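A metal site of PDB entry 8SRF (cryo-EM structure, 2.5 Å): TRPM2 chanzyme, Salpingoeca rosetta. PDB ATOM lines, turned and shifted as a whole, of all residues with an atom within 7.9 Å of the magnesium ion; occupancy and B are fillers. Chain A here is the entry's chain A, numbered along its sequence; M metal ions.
The side-chain hydroxyl (OG) of Ser 626 is in hydrogen-bond range of the side-chain carboxylate (OE2) of Glu 1114.
Ile 622 touches the magnesium ion (O to MG, 3.4 Å). Of the 18 residues printed, 4 come within 4 Å of the magnesium ion.
The magnesium ion is bound by OE1 of Glu 1114 (2.1 Å), O of Gly 623 (2.2 Å) and O of Leu 621 (2.5 Å). Slightly farther from the magnesium ion lies the side-chain carboxylate (OE2) of Glu 1114 (2.7 Å).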
ATOM      1  N   PHE A 593     -15.481   8.120   5.781  1.00  0.00           N
ATOM      2  CA  PHE A 593     -16.628   8.164   4.879  1.00  0.00           C
ATOM      3  C   PHE A 593     -17.939   8.223   5.649  1.00  0.00           C
ATOM      4  O   PHE A 593     -18.844   8.945   5.218  1.00  0.00           O
ATOM      5  CB  PHE A 593     -16.573   6.943   3.952  1.00  0.00           C
ATOM      6  CG  PHE A 593     -17.753   6.807   3.054  1.00  0.00           C
ATOM      7  CD1 PHE A 593     -18.066   7.828   2.126  1.00  0.00           C
ATOM      8  CD2 PHE A 593     -18.543   5.648   3.094  1.00  0.00           C
ATOM      9  CE1 PHE A 593     -19.163   7.699   1.269  1.00  0.00           C
ATOM     10  CE2 PHE A 593     -19.643   5.498   2.246  1.00  0.00           C
ATOM     11  CZ  PHE A 593     -19.949   6.528   1.327  1.00  0.00           C
ATOM     12  N   ALA A 597     -20.610  11.119   5.683  1.00  0.00           N
ATOM     13  CA  ALA A 597     -21.907  10.775   5.107  1.00  0.00           C
ATOM     14  C   ALA A 597     -23.048  11.201   6.027  1.00  0.00           C
ATOM     15  O   ALA A 597     -24.023  11.814   5.558  1.00  0.00           O
ATOM     16  CB  ALA A 597     -21.982   9.274   4.820  1.00  0.00           C
ATOM     17  N   SER A 600     -23.028  15.182   6.457  1.00  0.00           N
ATOM     18  CA  SER A 600     -23.569  15.699   5.188  1.00  0.00           C
ATOM     19  C   SER A 600     -25.073  15.527   5.122  1.00  0.00           C
ATOM     20  O   SER A 600     -25.742  16.383   4.546  1.00  0.00           O
ATOM     21  CB  SER A 600     -22.925  14.997   4.013  1.00  0.00           C
ATOM     22  OG  SER A 600     -23.325  13.671   4.038  1.00  0.00           O
ATOM     23  N   HIS A 618     -25.019  20.104  -3.115  1.00  0.00           N
ATOM     24  CA  HIS A 618     -23.621  19.887  -2.713  1.00  0.00           C
ATOM     25  C   HIS A 618     -23.494  18.880  -1.558  1.00  0.00           C
ATOM     26  O   HIS A 618     -22.616  17.992  -1.610  1.00  0.00           O
ATOM     27  CB  HIS A 618     -22.918  21.187  -2.365  1.00  0.00           C
ATOM     28  CG  HIS A 618     -21.467  20.987  -2.058  1.00  0.00           C
ATOM     29  ND1 HIS A 618     -20.558  20.626  -3.022  1.00  0.00           N
ATOM     30  CD2 HIS A 618     -20.782  21.039  -0.891  1.00  0.00           C
ATOM     31  CE1 HIS A 618     -19.363  20.478  -2.478  1.00  0.00           C
ATOM     32  NE2 HIS A 618     -19.471  20.729  -1.190  1.00  0.00           N
ATOM     33  N   PHE A 619     -24.360  19.007  -0.523  1.00  0.00           N
ATOM     34  CA  PHE A 619     -24.350  18.051   0.590  1.00  0.00           C
ATOM     35  C   PHE A 619     -24.878  16.685   0.171  1.00  0.00           C
ATOM     36  O   PHE A 619     -24.517  15.677   0.780  1.00  0.00           O
ATOM     37  CB  PHE A 619     -25.103  18.540   1.830  1.00  0.00           C
ATOM     38  CG  PHE A 619     -24.489  19.741   2.502  1.00  0.00           C
ATOM     39  CD1 PHE A 619     -23.118  19.731   2.795  1.00  0.00           C
ATOM     40  CD2 PHE A 619     -25.286  20.779   2.993  1.00  0.00           C
ATOM     41  CE1 PHE A 619     -22.515  20.809   3.450  1.00  0.00           C
ATOM     42  CE2 PHE A 619     -24.709  21.866   3.660  1.00  0.00           C
ATOM     43  CZ  PHE A 619     -23.320  21.873   3.883  1.00  0.00           C
ATOM     44  N   TRP A 620     -25.807  16.662  -0.790  1.00  0.00           N
ATOM     45  CA  TRP A 620     -26.294  15.434  -1.405  1.00  0.00           C
ATOM     46  C   TRP A 620     -25.184  14.728  -2.176  1.00  0.00           C
ATOM     47  O   TRP A 620     -25.100  13.493  -2.157  1.00  0.00           O
ATOM     48  CB  TRP A 620     -27.483  15.776  -2.304  1.00  0.00           C
ATOM     49  CG  TRP A 620     -27.951  14.675  -3.207  1.00  0.00           C
ATOM     50  CD1 TRP A 620     -28.744  13.626  -2.857  1.00  0.00           C
ATOM     51  CD2 TRP A 620     -27.671  14.522  -4.596  1.00  0.00           C
ATOM     52  NE1 TRP A 620     -28.977  12.820  -3.942  1.00  0.00           N
ATOM     53  CE2 TRP A 620     -28.325  13.350  -5.032  1.00  0.00           C
ATOM     54  CE3 TRP A 620     -26.914  15.264  -5.528  1.00  0.00           C
ATOM     55  CZ2 TRP A 620     -28.258  12.896  -6.353  1.00  0.00           C
ATOM     56  CZ3 TRP A 620     -26.849  14.814  -6.840  1.00  0.00           C
ATOM     57  CH2 TRP A 620     -27.515  13.637  -7.232  1.00  0.00           C
ATOM     58  N   LEU A 621     -24.342  15.494  -2.905  1.00  0.00           N
ATOM     59  CA  LEU A 621     -23.219  14.905  -3.646  1.00  0.00           C
ATOM     60  C   LEU A 621     -22.095  14.340  -2.777  1.00  0.00           C
ATOM     61  O   LEU A 621     -21.524  13.302  -3.147  1.00  0.00           O
ATOM     62  CB  LEU A 621     -22.659  15.981  -4.597  1.00  0.00           C
ATOM     63  CG  LEU A 621     -21.348  15.824  -5.390  1.00  0.00           C
ATOM     64  CD1 LEU A 621     -21.268  14.619  -6.307  1.00  0.00           C
ATOM     65  CD2 LEU A 621     -21.075  17.109  -6.171  1.00  0.00           C
ATOM     66  N   ILE A 622     -21.714  15.030  -1.680  1.00  0.00           N
ATOM     67  CA  ILE A 622     -20.643  14.510  -0.801  1.00  0.00           C
ATOM     68  C   ILE A 622     -21.009  13.219  -0.052  1.00  0.00           C
ATOM     69  O   ILE A 622     -20.174  12.308   0.017  1.00  0.00           O
ATOM     70  CB  ILE A 622     -20.019  15.571   0.138  1.00  0.00           C
ATOM     71  CG1 ILE A 622     -21.024  16.299   1.005  1.00  0.00           C
ATOM     72  CG2 ILE A 622     -19.153  16.531  -0.716  1.00  0.00           C
ATOM     73  CD1 ILE A 622     -20.422  17.369   1.889  1.00  0.00           C
ATOM     74  N   GLY A 623     -22.224  13.118   0.487  1.00  0.00           N
ATOM     75  CA  GLY A 623     -22.671  11.962   1.233  1.00  0.00           C
ATOM     76  C   GLY A 623     -23.076  10.787   0.368  1.00  0.00           C
ATOM     77  O   GLY A 623     -22.848  10.749  -0.838  1.00  0.00           O
ATOM     78  N   ASP A 624     -23.722   9.807   1.006  1.00  0.00           N
ATOM     79  CA  ASP A 624     -24.146   8.630   0.261  1.00  0.00           C
ATOM     80  C   ASP A 624     -25.663   8.511   0.213  1.00  0.00           C
ATOM     81  O   ASP A 624     -26.379   9.381   0.732  1.00  0.00           O
ATOM     82  CB  ASP A 624     -23.479   7.374   0.835  1.00  0.00           C
ATOM     83  CG  ASP A 624     -24.027   6.915   2.201  1.00  0.00           C
ATOM     84  OD1 ASP A 624     -24.489   7.726   3.048  1.00  0.00           O
ATOM     85  OD2 ASP A 624     -24.005   5.689   2.436  1.00  0.00           O
ATOM     86  N   GLN A 625     -26.093   7.376  -0.384  1.00  0.00           N
ATOM     87  CA  GLN A 625     -27.481   6.966  -0.640  1.00  0.00           C
ATOM     88  C   GLN A 625     -28.217   8.039  -1.454  1.00  0.00           C
ATOM     89  O   GLN A 625     -29.258   8.539  -1.023  1.00  0.00           O
ATOM     90  CB  GLN A 625     -28.249   6.621   0.652  1.00  0.00           C
ATOM     91  CG  GLN A 625     -27.893   5.274   1.241  1.00  0.00           C
ATOM     92  CD  GLN A 625     -28.241   4.128   0.322  1.00  0.00           C
ATOM     93  OE1 GLN A 625     -29.312   4.099  -0.281  1.00  0.00           O
ATOM     94  NE2 GLN A 625     -27.326   3.163   0.212  1.00  0.00           N
ATOM     95  N   SER A 626     -27.625   8.368  -2.627  1.00  0.00           N
ATOM     96  CA  SER A 626     -27.957   9.523  -3.473  1.00  0.00           C
ATOM     97  C   SER A 626     -29.386   9.506  -4.016  1.00  0.00           C
ATOM     98  O   SER A 626     -30.056  10.556  -4.038  1.00  0.00           O
ATOM     99  CB  SER A 626     -26.955   9.609  -4.635  1.00  0.00           C
ATOM    100  OG  SER A 626     -25.625   9.714  -4.168  1.00  0.00           O
ATOM    101  N   THR A1110     -23.158   0.206  -2.848  1.00  0.00           N
ATOM    102  CA  THR A1110     -22.851   1.569  -2.385  1.00  0.00           C
ATOM    103  C   THR A1110     -21.768   2.253  -3.240  1.00  0.00           C
ATOM    104  O   THR A1110     -21.944   3.411  -3.664  1.00  0.00           O
ATOM    105  CB  THR A1110     -22.437   1.492  -0.905  1.00  0.00           C
ATOM    106  OG1 THR A1110     -23.551   1.042  -0.128  1.00  0.00           O
ATOM    107  CG2 THR A1110     -21.974   2.836  -0.347  1.00  0.00           C
ATOM    108  N   GLU A1113     -23.212   2.868  -6.788  1.00  0.00           N
ATOM    109  CA  GLU A1113     -24.141   4.002  -6.756  1.00  0.00           C
ATOM    110  C   GLU A1113     -23.401   5.339  -6.698  1.00  0.00           C
ATOM    111  O   GLU A1113     -23.799   6.292  -7.381  1.00  0.00           O
ATOM    112  CB  GLU A1113     -25.089   3.837  -5.557  1.00  0.00           C
ATOM    113  CG  GLU A1113     -26.136   4.921  -5.377  1.00  0.00           C
ATOM    114  CD  GLU A1113     -27.123   4.606  -4.267  1.00  0.00           C
ATOM    115  OE1 GLU A1113     -26.803   3.733  -3.426  1.00  0.00           O
ATOM    116  OE2 GLU A1113     -28.202   5.228  -4.227  1.00  0.00           O
ATOM    117  N   GLU A1114     -22.308   5.412  -5.896  1.00  0.00           N
ATOM    118  CA  GLU A1114     -21.471   6.617  -5.798  1.00  0.00           C
ATOM    119  C   GLU A1114     -20.725   6.913  -7.096  1.00  0.00           C
ATOM    120  O   GLU A1114     -20.620   8.095  -7.482  1.00  0.00           O
ATOM    121  CB  GLU A1114     -20.505   6.546  -4.616  1.00  0.00           C
ATOM    122  CG  GLU A1114     -21.254   6.691  -3.346  1.00  0.00           C
ATOM    123  CD  GLU A1114     -21.680   8.131  -3.162  1.00  0.00           C
ATOM    124  OE1 GLU A1114     -20.909   9.050  -3.494  1.00  0.00           O
ATOM    125  OE2 GLU A1114     -22.854   8.348  -2.843  1.00  0.00           O
ATOM    126  N   LEU A1115     -20.172   5.856  -7.732  1.00  0.00           N
ATOM    127  CA  LEU A1115     -19.463   5.956  -9.009  1.00  0.00           C
ATOM    128  C   LEU A1115     -20.403   6.438 -10.119  1.00  0.00           C
ATOM    129  O   LEU A1115     -20.043   7.342 -10.888  1.00  0.00           O
ATOM    130  CB  LEU A1115     -18.853   4.599  -9.373  1.00  0.00           C
ATOM    131  CG  LEU A1115     -18.127   4.492 -10.712  1.00  0.00           C
ATOM    132  CD1 LEU A1115     -16.740   5.081 -10.614  1.00  0.00           C
ATOM    133  CD2 LEU A1115     -18.073   3.051 -11.182  1.00  0.00           C
ATOM    134  N   THR A1117     -23.244   8.105  -9.583  1.00  0.00           N
ATOM    135  CA  THR A1117     -23.620   9.471  -9.196  1.00  0.00           C
ATOM    136  C   THR A1117     -22.625  10.490  -9.751  1.00  0.00           C
ATOM    137  O   THR A1117     -23.034  11.526 -10.317  1.00  0.00           O
ATOM    138  CB  THR A1117     -23.718   9.563  -7.677  1.00  0.00           C
ATOM    139  OG1 THR A1117     -24.609   8.544  -7.197  1.00  0.00           O
ATOM    140  CG2 THR A1117     -24.255  10.913  -7.224  1.00  0.00           C
ATOM    141  N   ASP A1118     -21.311  10.200  -9.574  1.00  0.00           N
ATOM    142  CA  ASP A1118     -20.225  11.029 -10.121  1.00  0.00           C
ATOM    143  C   ASP A1118     -20.241  11.054 -11.654  1.00  0.00           C
ATOM    144  O   ASP A1118     -19.978  12.107 -12.256  1.00  0.00           O
ATOM    145  CB  ASP A1118     -18.852  10.578  -9.622  1.00  0.00           C
ATOM    146  CG  ASP A1118     -18.726  10.631  -8.116  1.00  0.00           C
ATOM    147  OD1 ASP A1118     -19.131  11.654  -7.518  1.00  0.00           O
ATOM    148  OD2 ASP A1118     -18.127   9.710  -7.541  1.00  0.00           O
HETATM  149 MG    MG M   1     -21.738  10.842  -2.683  1.00  0.00          MG
